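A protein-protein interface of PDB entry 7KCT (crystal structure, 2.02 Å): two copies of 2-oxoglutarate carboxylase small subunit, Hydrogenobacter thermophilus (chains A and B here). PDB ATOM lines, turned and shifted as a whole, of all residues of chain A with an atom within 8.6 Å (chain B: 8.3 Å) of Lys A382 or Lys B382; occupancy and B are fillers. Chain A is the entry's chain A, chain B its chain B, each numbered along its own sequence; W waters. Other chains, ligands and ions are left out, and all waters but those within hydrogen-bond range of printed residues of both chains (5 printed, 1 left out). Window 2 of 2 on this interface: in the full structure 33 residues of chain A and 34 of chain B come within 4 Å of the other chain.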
ATOM      1  N   THR A  47     -26.607   4.620 -19.350  1.00  0.00           N
ATOM      2  CA  THR A  47     -26.251   3.312 -19.854  1.00  0.00           C
ATOM      3  C   THR A  47     -27.450   2.362 -19.908  1.00  0.00           C
ATOM      4  O   THR A  47     -27.248   1.181 -20.131  1.00  0.00           O
ATOM      5  CB  THR A  47     -25.162   2.667 -18.985  1.00  0.00           C
ATOM      6  OG1 THR A  47     -25.679   2.468 -17.658  1.00  0.00           O
ATOM      7  CG2 THR A  47     -23.938   3.546 -18.885  1.00  0.00           C
ATOM      8  N   ARG A  49     -30.443  -0.076 -20.822  1.00  0.00           N
ATOM      9  CA  ARG A  49     -30.637  -0.984 -21.950  1.00  0.00           C
ATOM     10  C   ARG A  49     -31.671  -0.468 -22.955  1.00  0.00           C
ATOM     11  O   ARG A  49     -31.491  -0.636 -24.170  1.00  0.00           O
ATOM     12  CB  ARG A  49     -31.033  -2.352 -21.409  1.00  0.00           C
ATOM     13  CG  ARG A  49     -31.277  -3.353 -22.476  1.00  0.00           C
ATOM     14  CD  ARG A  49     -30.073  -3.554 -23.378  1.00  0.00           C
ATOM     15  NE  ARG A  49     -28.807  -3.625 -22.639  1.00  0.00           N
ATOM     16  CZ  ARG A  49     -27.589  -3.676 -23.198  1.00  0.00           C
ATOM     17  NH1 ARG A  49     -27.414  -3.623 -24.525  1.00  0.00           N
ATOM     18  NH2 ARG A  49     -26.522  -3.708 -22.412  1.00  0.00           N
ATOM     19  N   THR A 362     -25.484  -2.062  -7.134  1.00  0.00           N
ATOM     20  CA  THR A 362     -25.049  -2.336  -8.502  1.00  0.00           C
ATOM     21  C   THR A 362     -24.951  -3.846  -8.723  1.00  0.00           C
ATOM     22  O   THR A 362     -24.364  -4.571  -7.918  1.00  0.00           O
ATOM     23  CB  THR A 362     -23.684  -1.682  -8.781  1.00  0.00           C
ATOM     24  OG1 THR A 362     -23.792  -0.267  -8.564  1.00  0.00           O
ATOM     25  CG2 THR A 362     -23.215  -1.980 -10.273  1.00  0.00           C
ATOM     26  N   ILE A 363     -25.531  -4.331  -9.809  1.00  0.00           N
ATOM     27  CA  ILE A 363     -25.487  -5.758 -10.089  1.00  0.00           C
ATOM     28  C   ILE A 363     -24.066  -6.138 -10.462  1.00  0.00           C
ATOM     29  O   ILE A 363     -23.445  -5.488 -11.312  1.00  0.00           O
ATOM     30  CB  ILE A 363     -26.478  -6.103 -11.214  1.00  0.00           C
ATOM     31  CG1 ILE A 363     -27.895  -5.891 -10.674  1.00  0.00           C
ATOM     32  CG2 ILE A 363     -26.291  -7.516 -11.655  1.00  0.00           C
ATOM     33  CD1 ILE A 363     -29.018  -6.379 -11.617  1.00  0.00           C
ATOM     34  N   GLU A 364     -23.547  -7.186  -9.822  1.00  0.00           N
ATOM     35  CA  GLU A 364     -22.217  -7.723 -10.078  1.00  0.00           C
ATOM     36  C   GLU A 364     -22.419  -8.981 -10.920  1.00  0.00           C
ATOM     37  O   GLU A 364     -22.492  -8.913 -12.151  1.00  0.00           O
ATOM     38  CB  GLU A 364     -21.486  -8.036  -8.763  1.00  0.00           C
ATOM     39  N   ARG A 365     -22.612 -10.119 -10.271  1.00  0.00           N
ATOM     40  CA  ARG A 365     -22.847 -11.346 -11.017  1.00  0.00           C
ATOM     41  C   ARG A 365     -24.264 -11.341 -11.594  1.00  0.00           C
ATOM     42  O   ARG A 365     -25.218 -10.894 -10.947  1.00  0.00           O
ATOM     43  CB  ARG A 365     -22.612 -12.577 -10.144  1.00  0.00           C
ATOM     44  CG  ARG A 365     -21.150 -12.794  -9.675  1.00  0.00           C
ATOM     45  CD  ARG A 365     -21.084 -13.789  -8.508  1.00  0.00           C
ATOM     46  NE  ARG A 365     -19.750 -13.818  -7.901  1.00  0.00           N
ATOM     47  N   TYR A 366     -24.394 -11.806 -12.837  1.00  0.00           N
ATOM     48  CA  TYR A 366     -25.705 -11.802 -13.486  1.00  0.00           C
ATOM     49  C   TYR A 366     -25.733 -12.907 -14.533  1.00  0.00           C
ATOM     50  O   TYR A 366     -24.972 -12.865 -15.504  1.00  0.00           O
ATOM     51  CB  TYR A 366     -25.994 -10.446 -14.124  1.00  0.00           C
ATOM     52  CG  TYR A 366     -27.417 -10.256 -14.515  1.00  0.00           C
ATOM     53  CD1 TYR A 366     -28.408 -10.090 -13.548  1.00  0.00           C
ATOM     54  CD2 TYR A 366     -27.795 -10.289 -15.831  1.00  0.00           C
ATOM     55  CE1 TYR A 366     -29.729  -9.905 -13.899  1.00  0.00           C
ATOM     56  CE2 TYR A 366     -29.125 -10.141 -16.201  1.00  0.00           C
ATOM     57  CZ  TYR A 366     -30.093  -9.966 -15.227  1.00  0.00           C
ATOM     58  OH  TYR A 366     -31.412  -9.805 -15.592  1.00  0.00           O
ATOM     59  N   TYR A 367     -26.582 -13.896 -14.328  1.00  0.00           N
ATOM     60  CA  TYR A 367     -26.758 -14.944 -15.321  1.00  0.00           C
ATOM     61  C   TYR A 367     -28.246 -15.180 -15.482  1.00  0.00           C
ATOM     62  O   TYR A 367     -28.925 -15.491 -14.501  1.00  0.00           O
ATOM     63  CB  TYR A 367     -26.075 -16.248 -14.934  1.00  0.00           C
ATOM     64  CG  TYR A 367     -26.493 -17.394 -15.850  1.00  0.00           C
ATOM     65  CD1 TYR A 367     -25.891 -17.582 -17.097  1.00  0.00           C
ATOM     66  CD2 TYR A 367     -27.517 -18.278 -15.476  1.00  0.00           C
ATOM     67  CE1 TYR A 367     -26.274 -18.663 -17.934  1.00  0.00           C
ATOM     68  CE2 TYR A 367     -27.914 -19.305 -16.283  1.00  0.00           C
ATOM     69  CZ  TYR A 367     -27.312 -19.484 -17.524  1.00  0.00           C
ATOM     70  OH  TYR A 367     -27.722 -20.554 -18.281  1.00  0.00           O
ATOM     71  N   VAL A 368     -28.738 -15.060 -16.713  1.00  0.00           N
ATOM     72  CA  VAL A 368     -30.146 -15.222 -17.053  1.00  0.00           C
ATOM     73  C   VAL A 368     -30.446 -16.668 -17.464  1.00  0.00           C
ATOM     74  O   VAL A 368     -29.852 -17.165 -18.429  1.00  0.00           O
ATOM     75  CB  VAL A 368     -30.502 -14.247 -18.191  1.00  0.00           C
ATOM     76  CG1 VAL A 368     -31.936 -14.381 -18.586  1.00  0.00           C
ATOM     77  CG2 VAL A 368     -30.233 -12.837 -17.775  1.00  0.00           C
ATOM     78  N   HIS A 378     -36.347  -8.487 -19.208  1.00  0.00           N
ATOM     79  CA  HIS A 378     -35.359  -7.875 -18.332  1.00  0.00           C
ATOM     80  C   HIS A 378     -34.595  -6.783 -19.081  1.00  0.00           C
ATOM     81  O   HIS A 378     -34.554  -6.743 -20.322  1.00  0.00           O
ATOM     82  CB  HIS A 378     -34.405  -8.953 -17.758  1.00  0.00           C
ATOM     83  CG  HIS A 378     -33.345  -9.388 -18.705  1.00  0.00           C
ATOM     84  ND1 HIS A 378     -32.005  -9.419 -18.362  1.00  0.00           N
ATOM     85  CD2 HIS A 378     -33.409  -9.751 -20.010  1.00  0.00           C
ATOM     86  CE1 HIS A 378     -31.294  -9.773 -19.422  1.00  0.00           C
ATOM     87  NE2 HIS A 378     -32.124  -9.997 -20.428  1.00  0.00           N
ATOM     88  N   ALA A 379     -33.995  -5.885 -18.312  1.00  0.00           N
ATOM     89  CA  ALA A 379     -33.212  -4.830 -18.927  1.00  0.00           C
ATOM     90  C   ALA A 379     -31.860  -4.676 -18.253  1.00  0.00           C
ATOM     91  O   ALA A 379     -31.294  -3.580 -18.252  1.00  0.00           O
ATOM     92  CB  ALA A 379     -33.968  -3.497 -18.915  1.00  0.00           C
ATOM     93  N   SER A 380     -31.330  -5.758 -17.710  1.00  0.00           N
ATOM     94  CA  SER A 380     -30.172  -5.731 -16.831  1.00  0.00           C
ATOM     95  C   SER A 380     -28.999  -6.517 -17.392  1.00  0.00           C
ATOM     96  O   SER A 380     -29.159  -7.415 -18.216  1.00  0.00           O
ATOM     97  CB  SER A 380     -30.508  -6.305 -15.447  1.00  0.00           C
ATOM     98  OG  SER A 380     -31.300  -5.374 -14.744  1.00  0.00           O
ATOM     99  N   SER A 381     -27.820  -6.113 -16.923  1.00  0.00           N
ATOM    100  CA  SER A 381     -26.504  -6.635 -17.229  1.00  0.00           C
ATOM    101  C   SER A 381     -25.625  -6.366 -16.012  1.00  0.00           C
ATOM    102  O   SER A 381     -25.939  -5.516 -15.173  1.00  0.00           O
ATOM    103  CB  SER A 381     -25.854  -5.954 -18.447  1.00  0.00           C
ATOM    104  OG  SER A 381     -26.413  -6.386 -19.666  1.00  0.00           O
ATOM    105  N   LYS A 382     -24.470  -7.016 -15.966  1.00  0.00           N
ATOM    106  CA  LYS A 382     -23.497  -6.619 -14.957  1.00  0.00           C
ATOM    107  C   LYS A 382     -23.324  -5.101 -14.994  1.00  0.00           C
ATOM    108  O   LYS A 382     -23.198  -4.498 -16.071  1.00  0.00           O
ATOM    109  CB  LYS A 382     -22.161  -7.309 -15.191  1.00  0.00           C
ATOM    110  CG  LYS A 382     -21.041  -6.649 -14.383  1.00  0.00           C
ATOM    111  CD  LYS A 382     -20.021  -7.607 -13.894  1.00  0.00           C
ATOM    112  CE  LYS A 382     -18.847  -6.872 -13.234  1.00  0.00           C
ATOM    113  NZ  LYS A 382     -17.755  -7.821 -12.842  1.00  0.00           N
ATOM    114  N   GLY A 383     -23.337  -4.480 -13.809  1.00  0.00           N
ATOM    115  CA  GLY A 383     -23.216  -3.040 -13.710  1.00  0.00           C
ATOM    116  C   GLY A 383     -24.522  -2.267 -13.717  1.00  0.00           C
ATOM    117  O   GLY A 383     -24.492  -1.038 -13.609  1.00  0.00           O
ATOM    118  N   TYR A 384     -25.661  -2.931 -13.891  1.00  0.00           N
ATOM    119  CA  TYR A 384     -26.943  -2.255 -13.785  1.00  0.00           C
ATOM    120  C   TYR A 384     -27.091  -1.662 -12.382  1.00  0.00           C
ATOM    121  O   TYR A 384     -26.909  -2.360 -11.382  1.00  0.00           O
ATOM    122  CB  TYR A 384     -28.076  -3.231 -14.069  1.00  0.00           C
ATOM    123  CG  TYR A 384     -29.443  -2.596 -13.866  1.00  0.00           C
ATOM    124  CD1 TYR A 384     -29.975  -1.725 -14.798  1.00  0.00           C
ATOM    125  CD2 TYR A 384     -30.179  -2.867 -12.727  1.00  0.00           C
ATOM    126  CE1 TYR A 384     -31.214  -1.120 -14.587  1.00  0.00           C
ATOM    127  CE2 TYR A 384     -31.421  -2.293 -12.511  1.00  0.00           C
ATOM    128  CZ  TYR A 384     -31.943  -1.423 -13.436  1.00  0.00           C
ATOM    129  OH  TYR A 384     -33.176  -0.855 -13.187  1.00  0.00           O
ATOM    130  N   GLU A 385     -27.428  -0.381 -12.306  1.00  0.00           N
ATOM    131  CA  GLU A 385     -27.548   0.317 -11.019  1.00  0.00           C
ATOM    132  C   GLU A 385     -29.015   0.405 -10.629  1.00  0.00           C
ATOM    133  O   GLU A 385     -29.830   0.888 -11.398  1.00  0.00           O
ATOM    134  CB  GLU A 385     -26.895   1.699 -11.144  1.00  0.00           C
ATOM    135  N   GLU A 419     -28.837 -16.215 -11.360  1.00  0.00           N
ATOM    136  CA  GLU A 419     -27.803 -15.664 -10.480  1.00  0.00           C
ATOM    137  C   GLU A 419     -27.822 -14.140 -10.563  1.00  0.00           C
ATOM    138  O   GLU A 419     -27.658 -13.582 -11.660  1.00  0.00           O
ATOM    139  CB  GLU A 419     -26.400 -16.171 -10.842  1.00  0.00           C
ATOM    140  CG  GLU A 419     -25.330 -15.628  -9.827  1.00  0.00           C
ATOM    141  CD  GLU A 419     -23.966 -16.254  -9.950  1.00  0.00           C
ATOM    142  OE1 GLU A 419     -23.171 -16.179  -8.974  1.00  0.00           O
ATOM    143  OE2 GLU A 419     -23.679 -16.772 -11.027  1.00  0.00           O
ATOM    144  N   SER A 421     -25.986 -11.095  -8.059  1.00  0.00           N
ATOM    145  CA  SER A 421     -25.327 -10.645  -6.842  1.00  0.00           C
ATOM    146  C   SER A 421     -25.148  -9.136  -6.905  1.00  0.00           C
ATOM    147  O   SER A 421     -25.178  -8.492  -7.968  1.00  0.00           O
ATOM    148  CB  SER A 421     -23.951 -11.324  -6.603  1.00  0.00           C
ATOM    149  OG  SER A 421     -23.018 -10.755  -7.464  1.00  0.00           O
ATOM    150  N   THR B  47     -15.176 -21.766 -12.642  1.00  0.00           N
ATOM    151  CA  THR B  47     -16.302 -20.839 -12.572  1.00  0.00           C
ATOM    152  C   THR B  47     -17.350 -21.057 -13.666  1.00  0.00           C
ATOM    153  O   THR B  47     -18.185 -20.181 -13.857  1.00  0.00           O
ATOM    154  CB  THR B  47     -15.850 -19.354 -12.727  1.00  0.00           C
ATOM    155  OG1 THR B  47     -15.361 -19.102 -14.067  1.00  0.00           O
ATOM    156  CG2 THR B  47     -14.716 -19.058 -11.726  1.00  0.00           C
ATOM    157  N   ARG B  49     -20.692 -22.200 -15.735  1.00  0.00           N
ATOM    158  CA  ARG B  49     -22.105 -22.152 -15.367  1.00  0.00           C
ATOM    159  C   ARG B  49     -22.637 -23.540 -15.037  1.00  0.00           C
ATOM    160  O   ARG B  49     -23.376 -23.720 -14.055  1.00  0.00           O
ATOM    161  CB  ARG B  49     -22.864 -21.475 -16.507  1.00  0.00           C
ATOM    162  CG  ARG B  49     -24.355 -21.312 -16.286  1.00  0.00           C
ATOM    163  CD  ARG B  49     -24.673 -20.591 -14.960  1.00  0.00           C
ATOM    164  NE  ARG B  49     -23.829 -19.412 -14.724  1.00  0.00           N
ATOM    165  CZ  ARG B  49     -23.790 -18.697 -13.586  1.00  0.00           C
ATOM    166  NH1 ARG B  49     -22.925 -17.701 -13.492  1.00  0.00           N
ATOM    167  NH2 ARG B  49     -24.602 -18.955 -12.550  1.00  0.00           N
ATOM    168  N   LYS B  52     -21.825 -24.322 -11.537  1.00  0.00           N
ATOM    169  CA  LYS B  52     -22.630 -23.629 -10.533  1.00  0.00           C
ATOM    170  C   LYS B  52     -24.071 -24.130 -10.509  1.00  0.00           C
ATOM    171  O   LYS B  52     -24.704 -24.108  -9.457  1.00  0.00           O
ATOM    172  CB  LYS B  52     -22.606 -22.137 -10.809  1.00  0.00           C
ATOM    173  CG  LYS B  52     -21.206 -21.554 -10.726  1.00  0.00           C
ATOM    174  CD  LYS B  52     -21.146 -20.170 -11.385  1.00  0.00           C
ATOM    175  CE  LYS B  52     -20.010 -19.323 -10.857  1.00  0.00           C
ATOM    176  NZ  LYS B  52     -20.396 -17.869 -10.795  1.00  0.00           N
ATOM    177  N   THR B 362     -12.113 -12.674 -23.882  1.00  0.00           N
ATOM    178  CA  THR B 362     -13.026 -12.695 -22.744  1.00  0.00           C
ATOM    179  C   THR B 362     -14.261 -11.834 -22.996  1.00  0.00           C
ATOM    180  O   THR B 362     -14.150 -10.674 -23.391  1.00  0.00           O
ATOM    181  CB  THR B 362     -12.320 -12.177 -21.476  1.00  0.00           C
ATOM    182  OG1 THR B 362     -11.155 -12.966 -21.213  1.00  0.00           O
ATOM    183  CG2 THR B 362     -13.257 -12.258 -20.320  1.00  0.00           C
ATOM    184  N   ILE B 363     -15.440 -12.382 -22.718  1.00  0.00           N
ATOM    185  CA  ILE B 363     -16.658 -11.598 -22.843  1.00  0.00           C
ATOM    186  C   ILE B 363     -16.641 -10.477 -21.811  1.00  0.00           C
ATOM    187  O   ILE B 363     -16.403 -10.711 -20.617  1.00  0.00           O
ATOM    188  CB  ILE B 363     -17.888 -12.496 -22.666  1.00  0.00           C
ATOM    189  CG1 ILE B 363     -17.946 -13.502 -23.820  1.00  0.00           C
ATOM    190  CG2 ILE B 363     -19.127 -11.667 -22.514  1.00  0.00           C
ATOM    191  CD1 ILE B 363     -19.165 -14.372 -23.836  1.00  0.00           C
ATOM    192  N   GLU B 364     -16.930  -9.267 -22.268  1.00  0.00           N
ATOM    193  CA  GLU B 364     -17.027  -8.101 -21.419  1.00  0.00           C
ATOM    194  C   GLU B 364     -18.501  -7.738 -21.369  1.00  0.00           C
ATOM    195  O   GLU B 364     -19.269  -8.302 -20.533  1.00  0.00           O
ATOM    196  CB  GLU B 364     -16.117  -7.016 -22.016  1.00  0.00           C
ATOM    197  N   ARG B 365     -19.010  -6.947 -22.292  1.00  0.00           N
ATOM    198  CA  ARG B 365     -20.434  -6.660 -22.240  1.00  0.00           C
ATOM    199  C   ARG B 365     -21.211  -7.898 -22.706  1.00  0.00           C
ATOM    200  O   ARG B 365     -20.745  -8.683 -23.544  1.00  0.00           O
ATOM    201  CB  ARG B 365     -20.763  -5.392 -23.022  1.00  0.00           C
ATOM    202  CG  ARG B 365     -20.051  -4.140 -22.478  1.00  0.00           C
ATOM    203  CD  ARG B 365     -20.591  -2.880 -23.079  1.00  0.00           C
ATOM    204  NE  ARG B 365     -20.049  -2.662 -24.399  1.00  0.00           N
ATOM    205  CZ  ARG B 365     -19.050  -1.828 -24.670  1.00  0.00           C
ATOM    206  NH1 ARG B 365     -18.481  -1.079 -23.712  1.00  0.00           N
ATOM    207  NH2 ARG B 365     -18.643  -1.702 -25.917  1.00  0.00           N
ATOM    208  N   TYR B 366     -22.319  -8.156 -22.023  1.00  0.00           N
ATOM    209  CA  TYR B 366     -23.130  -9.327 -22.336  1.00  0.00           C
ATOM    210  C   TYR B 366     -24.582  -9.066 -21.965  1.00  0.00           C
ATOM    211  O   TYR B 366     -24.938  -9.006 -20.783  1.00  0.00           O
ATOM    212  CB  TYR B 366     -22.597 -10.546 -21.603  1.00  0.00           C
ATOM    213  CG  TYR B 366     -23.188 -11.868 -22.075  1.00  0.00           C
ATOM    214  CD1 TYR B 366     -22.822 -12.409 -23.307  1.00  0.00           C
ATOM    215  CD2 TYR B 366     -24.129 -12.541 -21.332  1.00  0.00           C
ATOM    216  CE1 TYR B 366     -23.346 -13.617 -23.754  1.00  0.00           C
ATOM    217  CE2 TYR B 366     -24.673 -13.777 -21.778  1.00  0.00           C
ATOM    218  CZ  TYR B 366     -24.282 -14.293 -23.000  1.00  0.00           C
ATOM    219  OH  TYR B 366     -24.769 -15.507 -23.493  1.00  0.00           O
ATOM    220  N   TYR B 367     -25.431  -8.920 -22.960  1.00  0.00           N
ATOM    221  CA  TYR B 367     -26.853  -8.783 -22.677  1.00  0.00           C
ATOM    222  C   TYR B 367     -27.650  -9.744 -23.517  1.00  0.00           C
ATOM    223  O   TYR B 367     -27.581  -9.689 -24.749  1.00  0.00           O
ATOM    224  CB  TYR B 367     -27.376  -7.381 -22.945  1.00  0.00           C
ATOM    225  CG  TYR B 367     -28.895  -7.307 -22.925  1.00  0.00           C
ATOM    226  CD1 TYR B 367     -29.565  -7.219 -21.713  1.00  0.00           C
ATOM    227  CD2 TYR B 367     -29.646  -7.330 -24.104  1.00  0.00           C
ATOM    228  CE1 TYR B 367     -30.925  -7.117 -21.660  1.00  0.00           C
ATOM    229  CE2 TYR B 367     -31.049  -7.235 -24.070  1.00  0.00           C
ATOM    230  CZ  TYR B 367     -31.669  -7.136 -22.826  1.00  0.00           C
ATOM    231  OH  TYR B 367     -33.016  -7.057 -22.696  1.00  0.00           O
ATOM    232  N   HIS B 378     -27.746 -20.942 -23.295  1.00  0.00           N
ATOM    233  CA  HIS B 378     -26.403 -20.393 -23.158  1.00  0.00           C
ATOM    234  C   HIS B 378     -25.824 -20.692 -21.780  1.00  0.00           C
ATOM    235  O   HIS B 378     -26.539 -21.034 -20.833  1.00  0.00           O
ATOM    236  CB  HIS B 378     -26.416 -18.887 -23.457  1.00  0.00           C
ATOM    237  CG  HIS B 378     -26.931 -18.040 -22.341  1.00  0.00           C
ATOM    238  ND1 HIS B 378     -26.243 -16.947 -21.862  1.00  0.00           N
ATOM    239  CD2 HIS B 378     -28.018 -18.169 -21.548  1.00  0.00           C
ATOM    240  CE1 HIS B 378     -26.915 -16.401 -20.869  1.00  0.00           C
ATOM    241  NE2 HIS B 378     -27.972 -17.148 -20.627  1.00  0.00           N
ATOM    242  N   ALA B 379     -24.514 -20.543 -21.675  1.00  0.00           N
ATOM    243  CA  ALA B 379     -23.838 -20.772 -20.403  1.00  0.00           C
ATOM    244  C   ALA B 379     -22.857 -19.649 -20.113  1.00  0.00           C
ATOM    245  O   ALA B 379     -21.833 -19.854 -19.460  1.00  0.00           O
ATOM    246  CB  ALA B 379     -23.134 -22.121 -20.366  1.00  0.00           C
ATOM    247  N   SER B 380     -23.170 -18.463 -20.579  1.00  0.00           N
ATOM    248  CA  SER B 380     -22.213 -17.372 -20.581  1.00  0.00           C
ATOM    249  C   SER B 380     -22.640 -16.227 -19.675  1.00  0.00           C
ATOM    250  O   SER B 380     -23.822 -16.028 -19.362  1.00  0.00           O
ATOM    251  CB  SER B 380     -22.011 -16.819 -21.982  1.00  0.00           C
ATOM    252  OG  SER B 380     -21.233 -17.692 -22.766  1.00  0.00           O
ATOM    253  N   SER B 381     -21.615 -15.482 -19.266  1.00  0.00           N
ATOM    254  CA  SER B 381     -21.717 -14.290 -18.441  1.00  0.00           C
ATOM    255  C   SER B 381     -20.481 -13.464 -18.755  1.00  0.00           C
ATOM    256  O   SER B 381     -19.508 -13.984 -19.309  1.00  0.00           O
ATOM    257  CB  SER B 381     -21.721 -14.604 -16.944  1.00  0.00           C
ATOM    258  OG  SER B 381     -22.838 -15.340 -16.557  1.00  0.00           O
ATOM    259  N   LYS B 382     -20.502 -12.188 -18.360  1.00  0.00           N
ATOM    260  CA  LYS B 382     -19.262 -11.420 -18.366  1.00  0.00           C
ATOM    261  C   LYS B 382     -18.164 -12.233 -17.704  1.00  0.00           C
ATOM    262  O   LYS B 382     -18.398 -12.899 -16.694  1.00  0.00           O
ATOM    263  CB  LYS B 382     -19.434 -10.081 -17.635  1.00  0.00           C
ATOM    264  CG  LYS B 382     -18.126  -9.387 -17.288  1.00  0.00           C
ATOM    265  CD  LYS B 382     -18.264  -7.889 -17.212  1.00  0.00           C
ATOM    266  CE  LYS B 382     -16.889  -7.249 -16.948  1.00  0.00           C
ATOM    267  NZ  LYS B 382     -16.087  -8.125 -16.006  1.00  0.00           N
ATOM    268  N   GLY B 383     -16.954 -12.168 -18.276  1.00  0.00           N
ATOM    269  CA  GLY B 383     -15.825 -12.901 -17.753  1.00  0.00           C
ATOM    270  C   GLY B 383     -15.671 -14.314 -18.295  1.00  0.00           C
ATOM    271  O   GLY B 383     -14.661 -14.963 -18.004  1.00  0.00           O
ATOM    272  N   TYR B 384     -16.634 -14.833 -19.045  1.00  0.00           N
ATOM    273  CA  TYR B 384     -16.451 -16.153 -19.675  1.00  0.00           C
ATOM    274  C   TYR B 384     -15.276 -16.112 -20.657  1.00  0.00           C
ATOM    275  O   TYR B 384     -15.172 -15.185 -21.444  1.00  0.00           O
ATOM    276  CB  TYR B 384     -17.745 -16.549 -20.383  1.00  0.00           C
ATOM    277  CG  TYR B 384     -17.670 -17.847 -21.159  1.00  0.00           C
ATOM    278  CD1 TYR B 384     -17.965 -19.056 -20.566  1.00  0.00           C
ATOM    279  CD2 TYR B 384     -17.313 -17.847 -22.521  1.00  0.00           C
ATOM    280  CE1 TYR B 384     -17.906 -20.251 -21.304  1.00  0.00           C
ATOM    281  CE2 TYR B 384     -17.236 -19.037 -23.259  1.00  0.00           C
ATOM    282  CZ  TYR B 384     -17.547 -20.236 -22.642  1.00  0.00           C
ATOM    283  OH  TYR B 384     -17.490 -21.433 -23.341  1.00  0.00           O
ATOM    284  N   GLU B 385     -14.329 -17.039 -20.568  1.00  0.00           N
ATOM    285  CA  GLU B 385     -13.182 -17.009 -21.465  1.00  0.00           C
ATOM    286  C   GLU B 385     -13.358 -18.013 -22.583  1.00  0.00           C
ATOM    287  O   GLU B 385     -13.777 -19.148 -22.341  1.00  0.00           O
ATOM    288  CB  GLU B 385     -11.815 -17.321 -20.884  1.00  0.00           C
ATOM    289  CG  GLU B 385     -11.135 -16.089 -20.290  1.00  0.00           C
ATOM    290  CD  GLU B 385      -9.666 -16.234 -19.979  1.00  0.00           C
ATOM    291  OE1 GLU B 385      -8.878 -16.086 -20.921  1.00  0.00           O
ATOM    292  OE2 GLU B 385      -9.337 -16.894 -18.972  1.00  0.00           O
ATOM    293  N   SER B 421     -19.444  -8.190 -26.224  1.00  0.00           N
ATOM    294  CA  SER B 421     -18.203  -7.537 -26.600  1.00  0.00           C
ATOM    295  C   SER B 421     -17.066  -8.271 -25.930  1.00  0.00           C
ATOM    296  O   SER B 421     -17.270  -9.090 -25.023  1.00  0.00           O
ATOM    297  CB  SER B 421     -18.200  -6.044 -26.230  1.00  0.00           C
ATOM    298  OG  SER B 421     -17.889  -5.868 -24.868  1.00  0.00           O
HETATM  299  O   HOH W   1     -22.381 -14.312 -13.608  1.00  0.00           O
HETATM  300  O   HOH W   2     -25.553 -13.979 -18.311  1.00  0.00           O
HETATM  301  O   HOH W   3     -23.624  -8.719 -18.117  1.00  0.00           O
HETATM  302  O   HOH W   4     -23.905  -5.466 -20.996  1.00  0.00           O
HETATM  303  O   HOH W   5     -27.704  -9.608 -19.582  1.00  0.00           O
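The backbone carbonyl oxygen of His B378 is in hydrogen-bond range of the side-chain hydroxyl of Tyr A367 (2.9 Å). A ring nitrogen (NE2) of His B378 is in hydrogen-bond range of the backbone carbonyl oxygen (O) of Val A368, 2.9 Å away. The backbone carbonyl oxygen (O) of Tyr A366 sits at hydrogen-bond distance from the side-chain hydroxyl (OG) of Ser B381 (3.4 Å). OE2 of Glu A419 is in salt-bridge range of NZ of Lys B52. O of His A378 lies within hydrogen-bond range of OH of Tyr B367 (2.8 Å). OG of Ser A381 lies within hydrogen-bond range of O of Tyr B366 (3.2 Å). OE2 of Glu A419 lies within salt-bridge range of NH1 of Arg B49 (2.7 Å).
A ring nitrogen (ND1) of His A378 sits close to the backbone carbonyl oxygen (O) of Ser A380, at 3.5 Å. N of Tyr A367 lies within hydrogen-bond range of O of Glu A419. ND1 of His A378 lies within hydrogen-bond range of OH of Tyr A366, 2.9 Å away. OH of Tyr B366 sits at hydrogen-bond distance from ND1 of His B378 (2.6 Å).
Among the printed residues, merely in contact across the chains: Arg A49 with Tyr B367, Tyr A367 with Arg B49, Tyr A367 with Ser B380, Tyr A367 with Ser B381, Ser A380 with Tyr B367, Ser A381 with Tyr B367 and Lys A382 with Lys B382.
Printed residues of chain B within 4 Å of Lys A382: Lys B382. Lys B382 touches just one residue of chain A: Lys A382 (3.6 Å). Ser B381 touches just these residues of chain A: Tyr A366 (3.4 Å) and Tyr A367 (3.7 Å). No residue of chain A comes within 4 Å of Gly B383. Of the printed residues of chain A, Ser B380 touches Tyr A367. Of the printed residues of chain A, His B378 touches Tyr A367 (2.9 Å) and Val A368 (2.9 Å). Of the printed residues of chain B, Arg A49 touches Tyr B367. Printed residues of chain A within 4 Å of Lys B52: Glu A419.
Printed residues of chain A that touch a printed residue of chain B: Arg A49, Tyr A366, Tyr A367, Val A368, His A378, Ser A380, Ser A381, Lys A382 and Glu A419. Hydrophobic or aromatic side chains of chain B that line the printed part of chain A: Tyr B367 and His B378. Among the printed residues, 14 pairs touch across the chains. Among the printed residues, Asp or Glu carboxylates within 4 Å of a Lys or Arg side-chain nitrogen of the other chain: Glu A419 with Arg B49 and Glu A419 with Lys B52.
Tyr A366 touches Ser B381, and with the chains exchanged Ser A381 touches Tyr B366. Tyr A367 touches His B378, and with the chains exchanged His A378 touches Tyr B367. Tyr A367 touches Ser B380, and with the chains exchanged Ser A380 touches Tyr B367. Lys A382 touches its own counterpart, Lys B382. Of the 14 pairs that touch across the chains among the printed residues, 11 have their exchanged pair printed and touching as well.
Water W3 lies within hydrogen-bond range of N of Lys A382 (2.9 Å) and O of Tyr B366 (3.0 Å). Water W2 bridges O of Ser B380 (2.9 Å) and O of Tyr A366 (3.1 Å). Water W5 lies within hydrogen-bond range of O of Ser A380 (3.0 Å), O of Tyr B366 (3.1 Å) and OG of Ser A381 (3.5 Å). Water W4 lies within hydrogen-bond range of OG of Ser A381 (3.0 Å), N of Tyr B366 (3.3 Å) and NH2 of Arg A49 (3.5 Å). Water W1 lies within hydrogen-bond range of OG of Ser B381 (3.2 Å), N of Tyr A366 (3.3 Å) and NH1 of Arg B49 (3.4 Å).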
